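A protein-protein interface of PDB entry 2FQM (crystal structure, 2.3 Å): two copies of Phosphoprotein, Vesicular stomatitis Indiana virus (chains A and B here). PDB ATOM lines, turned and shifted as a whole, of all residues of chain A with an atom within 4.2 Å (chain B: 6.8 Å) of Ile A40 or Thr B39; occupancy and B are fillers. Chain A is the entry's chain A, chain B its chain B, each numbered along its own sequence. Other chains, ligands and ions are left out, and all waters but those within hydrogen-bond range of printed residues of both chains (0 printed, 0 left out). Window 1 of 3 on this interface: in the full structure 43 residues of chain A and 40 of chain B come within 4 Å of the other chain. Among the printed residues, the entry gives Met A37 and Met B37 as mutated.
Trp A36 touches Thr B39, and with the chains exchanged Thr A39 touches Trp B36. Ile A40 touches Thr B39, but with the chains exchanged Thr A39 does not touch Ile B40 (4.6 Å). Val A43 touches Ile B40, but with the chains exchanged Ile A40 does not touch Val B43 (4.3 Å). Val B43 touches its own counterpart, Val A43. Of the 19 pairs that touch across the chains among the printed residues, 4 have their exchanged pair printed and touching as well.
Of the printed residues of chain B, Trp A6 touches Gln B35, Leu B38 and Thr B39. Printed residues of chain B within 4 Å of Pro A9: Leu B38 and Ala B42. Printed residues of chain B within 4 Å of Ile A40: Thr B39. Of the printed residues of chain B, Ala A42 touches Leu B22 (3.99 Å). Of the printed residues of chain A, Leu B38 touches Trp A6 and Pro A9. Thr B39 touches just these residues of chain A: Trp A6, Thr A23, Trp A36 and Ile A40. Printed residues of chain A within 4 Å of Val B43: Val A43 (3.5 Å). The nearest printed residue of chain A that does not touch Trp B36 is Trp A6 (5.2 Å).
NE1 of Trp A6 lies within hydrogen-bond range of O of Thr A23 (3.3 Å). O of Trp B36 is in hydrogen-bond range of OG1 of Thr B39 (2.7 Å).
OG1 of Thr B39 sits at hydrogen-bond distance from NE1 of Trp A36, at 2.9 Å.
Hydrophobic or aromatic side chains of chain B within 4 Å of the printed part of chain A: Leu B22, Trp B36, Leu B38, Ile B40, Ala B42, Val B43, Val B44, Phe B57 and Val B64. Of the 12 printed residues of chain A, 10 touch a printed residue of chain B. Printed residues of chain A that touch a printed residue of chain B: Trp A6, Pro A9, Thr A23, Trp A36, Met A37, Thr A39, Ile A40, Lys A41, Ala A42 and Val A43. Among the printed residues, no Asp or Glu carboxylate lies within 4 Å of a Lys or Arg side-chain nitrogen of the other chain.
Among the printed residues, merely in contact across the chains: Trp A6 with Gln B35, Trp A6 with Leu B38, Trp A6 with Thr B39, Pro A9 with Leu B38, Pro A9 with Ala B42, Thr A23 with Thr B39, Trp A36 with Trp B36, Trp A36 with Val B64, Met A37 with Phe B57, Met A37 with Val B64, Thr A39 with Trp B36, Ile A40 with Thr B39, Lys A41 with Phe B57, Ala A42 with Leu B22, Val A43 with Leu B22, Val A43 with Ile B40, Val A43 with Val B43 and Val A43 with Val B44.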
ATOM      1  N   TRP A   6      19.787  18.238   0.030  1.00  0.00           N
ATOM      2  CA  TRP A   6      20.013  18.778  -1.314  1.00  0.00           C
ATOM      3  C   TRP A   6      21.374  18.257  -1.814  1.00  0.00           C
ATOM      4  O   TRP A   6      22.366  18.523  -1.154  1.00  0.00           O
ATOM      5  CB  TRP A   6      20.095  20.314  -1.245  1.00  0.00           C
ATOM      6  CG  TRP A   6      20.461  20.913  -2.616  1.00  0.00           C
ATOM      7  CD1 TRP A   6      19.703  20.860  -3.757  1.00  0.00           C
ATOM      8  CD2 TRP A   6      21.678  21.592  -2.985  1.00  0.00           C
ATOM      9  NE1 TRP A   6      20.372  21.458  -4.805  1.00  0.00           N
ATOM     10  CE2 TRP A   6      21.578  21.918  -4.369  1.00  0.00           C
ATOM     11  CE3 TRP A   6      22.835  21.961  -2.286  1.00  0.00           C
ATOM     12  CZ2 TRP A   6      22.585  22.590  -5.064  1.00  0.00           C
ATOM     13  CZ3 TRP A   6      23.855  22.636  -2.982  1.00  0.00           C
ATOM     14  CH2 TRP A   6      23.721  22.943  -4.360  1.00  0.00           C
ATOM     15  N   PRO A   9      26.705  19.802  -6.476  1.00  0.00           N
ATOM     16  CA  PRO A   9      27.162  19.325  -7.793  1.00  0.00           C
ATOM     17  C   PRO A   9      28.121  18.179  -7.591  1.00  0.00           C
ATOM     18  O   PRO A   9      29.012  18.266  -6.751  1.00  0.00           O
ATOM     19  CB  PRO A   9      27.907  20.551  -8.365  1.00  0.00           C
ATOM     20  CG  PRO A   9      27.038  21.675  -7.880  1.00  0.00           C
ATOM     21  CD  PRO A   9      26.682  21.279  -6.426  1.00  0.00           C
ATOM     22  N   THR A  23      22.012  19.315  -9.242  1.00  0.00           N
ATOM     23  CA  THR A  23      20.682  19.208  -8.682  1.00  0.00           C
ATOM     24  C   THR A  23      19.987  20.565  -8.525  1.00  0.00           C
ATOM     25  O   THR A  23      20.564  21.574  -8.105  1.00  0.00           O
ATOM     26  CB  THR A  23      20.776  18.464  -7.334  1.00  0.00           C
ATOM     27  OG1 THR A  23      21.382  17.203  -7.600  1.00  0.00           O
ATOM     28  CG2 THR A  23      19.404  18.220  -6.701  1.00  0.00           C
ATOM     29  N   TRP A  36      16.146  28.565 -13.610  1.00  0.00           N
ATOM     30  CA  TRP A  36      17.377  27.960 -13.186  1.00  0.00           C
ATOM     31  C   TRP A  36      17.980  27.209 -14.386  1.00  0.00           C
ATOM     32  O   TRP A  36      19.159  27.331 -14.710  1.00  0.00           O
ATOM     33  CB  TRP A  36      17.101  26.984 -12.055  1.00  0.00           C
ATOM     34  CG  TRP A  36      18.300  26.259 -11.709  1.00  0.00           C
ATOM     35  CD1 TRP A  36      19.389  26.723 -10.938  1.00  0.00           C
ATOM     36  CD2 TRP A  36      18.634  24.943 -12.122  1.00  0.00           C
ATOM     37  NE1 TRP A  36      20.356  25.738 -10.869  1.00  0.00           N
ATOM     38  CE2 TRP A  36      19.923  24.645 -11.581  1.00  0.00           C
ATOM     39  CE3 TRP A  36      17.981  23.965 -12.897  1.00  0.00           C
ATOM     40  CZ2 TRP A  36      20.539  23.424 -11.787  1.00  0.00           C
ATOM     41  CZ3 TRP A  36      18.626  22.716 -13.105  1.00  0.00           C
ATOM     42  CH2 TRP A  36      19.866  22.470 -12.553  1.00  0.00           C
ATOM     43  N   MET A  37      17.144  26.454 -15.081  1.00  0.00           N
ATOM     44  CA  MET A  37      17.646  25.693 -16.214  1.00  0.00           C
ATOM     45  C   MET A  37      18.237  26.613 -17.310  1.00  0.00           C
ATOM     46  O   MET A  37      19.182  26.251 -17.962  1.00  0.00           O
ATOM     47  CB  MET A  37      16.520  24.797 -16.802  1.00  0.00           C
ATOM     48  CG  MET A  37      16.911  24.148 -18.130  1.00  0.00           C
ATOM     49  SD  MET A  37      18.328  23.008 -17.959  1.00  0.00           S
ATOM     50  CE  MET A  37      17.599  21.562 -17.793  1.00  0.00           C
ATOM     51  N   LEU A  38      17.668  27.792 -17.505  1.00  0.00           N
ATOM     52  CA  LEU A  38      18.130  28.725 -18.542  1.00  0.00           C
ATOM     53  C   LEU A  38      19.433  29.378 -18.144  1.00  0.00           C
ATOM     54  O   LEU A  38      20.260  29.672 -18.969  1.00  0.00           O
ATOM     55  CB  LEU A  38      17.045  29.794 -18.800  1.00  0.00           C
ATOM     56  CG  LEU A  38      15.770  29.269 -19.504  1.00  0.00           C
ATOM     57  CD1 LEU A  38      14.742  30.312 -19.545  1.00  0.00           C
ATOM     58  CD2 LEU A  38      16.069  28.915 -20.967  1.00  0.00           C
ATOM     59  N   THR A  39      19.594  29.657 -16.864  1.00  0.00           N
ATOM     60  CA  THR A  39      20.854  30.246 -16.307  1.00  0.00           C
ATOM     61  C   THR A  39      22.007  29.202 -16.606  1.00  0.00           C
ATOM     62  O   THR A  39      23.062  29.547 -17.123  1.00  0.00           O
ATOM     63  CB  THR A  39      20.636  30.441 -14.726  1.00  0.00           C
ATOM     64  OG1 THR A  39      19.812  31.596 -14.499  1.00  0.00           O
ATOM     65  CG2 THR A  39      21.928  30.560 -13.975  1.00  0.00           C
ATOM     66  N   ILE A  40      21.791  27.927 -16.256  1.00  0.00           N
ATOM     67  CA  ILE A  40      22.788  26.897 -16.484  1.00  0.00           C
ATOM     68  C   ILE A  40      22.992  26.897 -18.001  1.00  0.00           C
ATOM     69  O   ILE A  40      24.127  26.925 -18.478  1.00  0.00           O
ATOM     70  CB  ILE A  40      22.289  25.436 -16.054  1.00  0.00           C
ATOM     71  CG1 ILE A  40      22.330  25.203 -14.516  1.00  0.00           C
ATOM     72  CG2 ILE A  40      23.093  24.371 -16.746  1.00  0.00           C
ATOM     73  CD1 ILE A  40      23.268  26.113 -13.636  1.00  0.00           C
ATOM     74  N   LYS A  41      21.919  26.872 -18.782  1.00  0.00           N
ATOM     75  CA  LYS A  41      22.094  26.882 -20.235  1.00  0.00           C
ATOM     76  C   LYS A  41      22.876  28.133 -20.736  1.00  0.00           C
ATOM     77  O   LYS A  41      23.698  27.991 -21.600  1.00  0.00           O
ATOM     78  CB  LYS A  41      20.745  26.730 -20.944  1.00  0.00           C
ATOM     79  CG  LYS A  41      20.879  26.566 -22.449  1.00  0.00           C
ATOM     80  CD  LYS A  41      19.532  26.801 -23.230  1.00  0.00           C
ATOM     81  CE  LYS A  41      19.757  27.148 -24.753  1.00  0.00           C
ATOM     82  NZ  LYS A  41      20.006  25.923 -25.537  1.00  0.00           N
ATOM     83  N   ALA A  42      22.655  29.339 -20.191  1.00  0.00           N
ATOM     84  CA  ALA A  42      23.427  30.528 -20.602  1.00  0.00           C
ATOM     85  C   ALA A  42      24.910  30.375 -20.283  1.00  0.00           C
ATOM     86  O   ALA A  42      25.794  30.925 -20.987  1.00  0.00           O
ATOM     87  CB  ALA A  42      22.906  31.801 -19.897  1.00  0.00           C
ATOM     88  N   VAL A  43      25.201  29.640 -19.208  1.00  0.00           N
ATOM     89  CA  VAL A  43      26.606  29.457 -18.865  1.00  0.00           C
ATOM     90  C   VAL A  43      27.273  28.479 -19.820  1.00  0.00           C
ATOM     91  O   VAL A  43      28.340  28.803 -20.300  1.00  0.00           O
ATOM     92  CB  VAL A  43      26.827  29.024 -17.391  1.00  0.00           C
ATOM     93  CG1 VAL A  43      28.357  28.835 -17.151  1.00  0.00           C
ATOM     94  CG2 VAL A  43      26.295  30.124 -16.436  1.00  0.00           C
ATOM     95  N   VAL A  44      26.663  27.319 -20.156  1.00  0.00           N
ATOM     96  CA  VAL A  44      27.392  26.481 -21.084  1.00  0.00           C
ATOM     97  C   VAL A  44      27.572  27.184 -22.408  1.00  0.00           C
ATOM     98  O   VAL A  44      28.628  27.146 -22.987  1.00  0.00           O
ATOM     99  CB  VAL A  44      26.853  24.975 -21.215  1.00  0.00           C
ATOM    100  CG1 VAL A  44      25.889  24.708 -20.209  1.00  0.00           C
ATOM    101  CG2 VAL A  44      26.477  24.611 -22.601  1.00  0.00           C
ATOM    102  N   LEU B  22      23.779  37.426 -15.043  1.00  0.00           N
ATOM    103  CA  LEU B  22      22.736  36.455 -14.819  1.00  0.00           C
ATOM    104  C   LEU B  22      21.993  36.848 -13.602  1.00  0.00           C
ATOM    105  O   LEU B  22      22.597  37.098 -12.568  1.00  0.00           O
ATOM    106  CB  LEU B  22      23.369  35.087 -14.623  1.00  0.00           C
ATOM    107  CG  LEU B  22      24.191  34.681 -15.843  1.00  0.00           C
ATOM    108  CD1 LEU B  22      24.844  33.352 -15.600  1.00  0.00           C
ATOM    109  CD2 LEU B  22      23.279  34.595 -17.070  1.00  0.00           C
ATOM    110  N   SER B  34      22.151  30.197  -2.296  1.00  0.00           N
ATOM    111  CA  SER B  34      23.472  29.598  -2.313  1.00  0.00           C
ATOM    112  C   SER B  34      23.515  28.357  -3.220  1.00  0.00           C
ATOM    113  O   SER B  34      24.426  28.213  -4.020  1.00  0.00           O
ATOM    114  CB  SER B  34      23.933  29.245  -0.892  1.00  0.00           C
ATOM    115  OG  SER B  34      24.361  30.411  -0.209  1.00  0.00           O
ATOM    116  N   GLN B  35      22.531  27.474  -3.097  1.00  0.00           N
ATOM    117  CA  GLN B  35      22.448  26.259  -3.917  1.00  0.00           C
ATOM    118  C   GLN B  35      22.510  26.641  -5.399  1.00  0.00           C
ATOM    119  O   GLN B  35      23.243  26.071  -6.170  1.00  0.00           O
ATOM    120  CB  GLN B  35      21.137  25.534  -3.639  1.00  0.00           C
ATOM    121  CG  GLN B  35      20.951  25.131  -2.199  1.00  0.00           C
ATOM    122  CD  GLN B  35      19.569  24.612  -1.904  1.00  0.00           C
ATOM    123  OE1 GLN B  35      18.610  24.841  -2.650  1.00  0.00           O
ATOM    124  NE2 GLN B  35      19.451  23.922  -0.798  1.00  0.00           N
ATOM    125  N   TRP B  36      21.761  27.667  -5.754  1.00  0.00           N
ATOM    126  CA  TRP B  36      21.690  28.130  -7.113  1.00  0.00           C
ATOM    127  C   TRP B  36      23.068  28.567  -7.572  1.00  0.00           C
ATOM    128  O   TRP B  36      23.539  28.170  -8.612  1.00  0.00           O
ATOM    129  CB  TRP B  36      20.746  29.311  -7.164  1.00  0.00           C
ATOM    130  CG  TRP B  36      20.339  29.778  -8.547  1.00  0.00           C
ATOM    131  CD1 TRP B  36      21.151  30.180  -9.563  1.00  0.00           C
ATOM    132  CD2 TRP B  36      19.005  29.918  -9.029  1.00  0.00           C
ATOM    133  NE1 TRP B  36      20.400  30.569 -10.668  1.00  0.00           N
ATOM    134  CE2 TRP B  36      19.080  30.404 -10.365  1.00  0.00           C
ATOM    135  CE3 TRP B  36      17.752  29.684  -8.465  1.00  0.00           C
ATOM    136  CZ2 TRP B  36      17.955  30.645 -11.143  1.00  0.00           C
ATOM    137  CZ3 TRP B  36      16.606  29.934  -9.250  1.00  0.00           C
ATOM    138  CH2 TRP B  36      16.725  30.405 -10.578  1.00  0.00           C
ATOM    139  N   MET B  37      23.695  29.390  -6.754  1.00  0.00           N
ATOM    140  CA  MET B  37      24.978  29.952  -7.040  1.00  0.00           C
ATOM    141  C   MET B  37      26.016  28.887  -7.206  1.00  0.00           C
ATOM    142  O   MET B  37      26.872  28.925  -8.098  1.00  0.00           O
ATOM    143  CB  MET B  37      25.356  30.854  -5.903  1.00  0.00           C
ATOM    144  CG  MET B  37      24.429  32.028  -5.756  1.00  0.00           C
ATOM    145  SD  MET B  37      24.826  33.263  -6.927  1.00  0.00           S
ATOM    146  CE  MET B  37      24.763  34.708  -5.874  1.00  0.00           C
ATOM    147  N   LEU B  38      25.944  27.935  -6.311  1.00  0.00           N
ATOM    148  CA  LEU B  38      26.835  26.807  -6.320  1.00  0.00           C
ATOM    149  C   LEU B  38      26.644  26.023  -7.606  1.00  0.00           C
ATOM    150  O   LEU B  38      27.609  25.523  -8.120  1.00  0.00           O
ATOM    151  CB  LEU B  38      26.520  25.867  -5.166  1.00  0.00           C
ATOM    152  CG  LEU B  38      27.573  25.410  -4.192  1.00  0.00           C
ATOM    153  CD1 LEU B  38      26.983  24.296  -3.376  1.00  0.00           C
ATOM    154  CD2 LEU B  38      28.814  24.966  -4.934  1.00  0.00           C
ATOM    155  N   THR B  39      25.419  25.881  -8.121  1.00  0.00           N
ATOM    156  CA  THR B  39      25.290  25.076  -9.339  1.00  0.00           C
ATOM    157  C   THR B  39      25.898  25.810 -10.498  1.00  0.00           C
ATOM    158  O   THR B  39      26.475  25.180 -11.383  1.00  0.00           O
ATOM    159  CB  THR B  39      23.869  24.727  -9.762  1.00  0.00           C
ATOM    160  OG1 THR B  39      23.156  25.932 -10.016  1.00  0.00           O
ATOM    161  CG2 THR B  39      23.142  23.917  -8.685  1.00  0.00           C
ATOM    162  N   ILE B  40      25.876  27.142 -10.477  1.00  0.00           N
ATOM    163  CA  ILE B  40      26.445  27.788 -11.634  1.00  0.00           C
ATOM    164  C   ILE B  40      27.960  27.759 -11.623  1.00  0.00           C
ATOM    165  O   ILE B  40      28.604  27.640 -12.649  1.00  0.00           O
ATOM    166  CB  ILE B  40      25.878  29.247 -11.894  1.00  0.00           C
ATOM    167  CG1 ILE B  40      27.020  30.072 -12.457  1.00  0.00           C
ATOM    168  CG2 ILE B  40      25.106  29.802 -10.736  1.00  0.00           C
ATOM    169  CD1 ILE B  40      26.624  31.457 -12.763  1.00  0.00           C
ATOM    170  N   LYS B  41      28.520  27.868 -10.438  1.00  0.00           N
ATOM    171  CA  LYS B  41      29.939  27.831 -10.274  1.00  0.00           C
ATOM    172  C   LYS B  41      30.494  26.436 -10.686  1.00  0.00           C
ATOM    173  O   LYS B  41      31.647  26.315 -11.245  1.00  0.00           O
ATOM    174  CB  LYS B  41      30.280  28.134  -8.801  1.00  0.00           C
ATOM    175  CG  LYS B  41      31.725  28.364  -8.515  1.00  0.00           C
ATOM    176  CD  LYS B  41      31.954  28.819  -7.087  1.00  0.00           C
ATOM    177  CE  LYS B  41      33.417  29.196  -6.895  1.00  0.00           C
ATOM    178  NZ  LYS B  41      33.841  29.190  -5.473  1.00  0.00           N
ATOM    179  N   ALA B  42      29.741  25.368 -10.381  1.00  0.00           N
ATOM    180  CA  ALA B  42      30.197  24.028 -10.790  1.00  0.00           C
ATOM    181  C   ALA B  42      30.338  24.025 -12.308  1.00  0.00           C
ATOM    182  O   ALA B  42      31.270  23.444 -12.841  1.00  0.00           O
ATOM    183  CB  ALA B  42      29.204  22.955 -10.349  1.00  0.00           C
ATOM    184  N   VAL B  43      29.433  24.714 -13.023  1.00  0.00           N
ATOM    185  CA  VAL B  43      29.577  24.757 -14.496  1.00  0.00           C
ATOM    186  C   VAL B  43      30.785  25.567 -14.925  1.00  0.00           C
ATOM    187  O   VAL B  43      31.479  25.170 -15.834  1.00  0.00           O
ATOM    188  CB  VAL B  43      28.365  25.379 -15.225  1.00  0.00           C
ATOM    189  CG1 VAL B  43      28.650  25.359 -16.738  1.00  0.00           C
ATOM    190  CG2 VAL B  43      27.076  24.599 -14.884  1.00  0.00           C
ATOM    191  N   VAL B  44      31.015  26.730 -14.293  1.00  0.00           N
ATOM    192  CA  VAL B  44      32.184  27.476 -14.704  1.00  0.00           C
ATOM    193  C   VAL B  44      33.448  26.639 -14.397  1.00  0.00           C
ATOM    194  O   VAL B  44      34.333  26.561 -15.244  1.00  0.00           O
ATOM    195  CB  VAL B  44      32.266  28.898 -14.079  1.00  0.00           C
ATOM    196  CG1 VAL B  44      30.877  29.552 -14.162  1.00  0.00           C
ATOM    197  CG2 VAL B  44      32.774  28.837 -12.682  1.00  0.00           C
ATOM    198  N   PHE B  57      24.853  18.018 -23.150  1.00  0.00           N
ATOM    199  CA  PHE B  57      24.121  18.628 -22.099  1.00  0.00           C
ATOM    200  C   PHE B  57      22.635  18.185 -22.140  1.00  0.00           C
ATOM    201  O   PHE B  57      21.878  18.673 -22.986  1.00  0.00           O
ATOM    202  CB  PHE B  57      24.338  20.170 -22.259  1.00  0.00           C
ATOM    203  CG  PHE B  57      23.340  21.037 -21.480  1.00  0.00           C
ATOM    204  CD1 PHE B  57      23.035  20.756 -20.145  1.00  0.00           C
ATOM    205  CD2 PHE B  57      22.661  22.100 -22.104  1.00  0.00           C
ATOM    206  CE1 PHE B  57      22.064  21.489 -19.443  1.00  0.00           C
ATOM    207  CE2 PHE B  57      21.689  22.838 -21.410  1.00  0.00           C
ATOM    208  CZ  PHE B  57      21.394  22.526 -20.073  1.00  0.00           C
ATOM    209  N   VAL B  64      20.172  18.809 -14.088  1.00  0.00           N
ATOM    210  CA  VAL B  64      20.897  18.658 -15.343  1.00  0.00           C
ATOM    211  C   VAL B  64      22.172  17.907 -15.248  1.00  0.00           C
ATOM    212  O   VAL B  64      22.813  17.874 -14.209  1.00  0.00           O
ATOM    213  CB  VAL B  64      21.258  20.024 -16.042  1.00  0.00           C
ATOM    214  CG1 VAL B  64      20.072  20.856 -16.255  1.00  0.00           C
ATOM    215  CG2 VAL B  64      22.260  20.753 -15.247  1.00  0.00           C
ATOM    216  N   ILE B  66      25.867  17.194 -17.517  1.00  0.00           N
ATOM    217  CA  ILE B  66      26.824  17.568 -18.535  1.00  0.00           C
ATOM    218  C   ILE B  66      27.729  16.402 -18.649  1.00  0.00           C
ATOM    219  O   ILE B  66      28.337  16.009 -17.666  1.00  0.00           O
ATOM    220  CB  ILE B  66      27.629  18.776 -18.129  1.00  0.00           C
ATOM    221  CG1 ILE B  66      26.662  19.921 -17.937  1.00  0.00           C
ATOM    222  CG2 ILE B  66      28.758  19.114 -19.219  1.00  0.00           C
ATOM    223  CD1 ILE B  66      27.265  21.196 -17.420  1.00  0.00           C
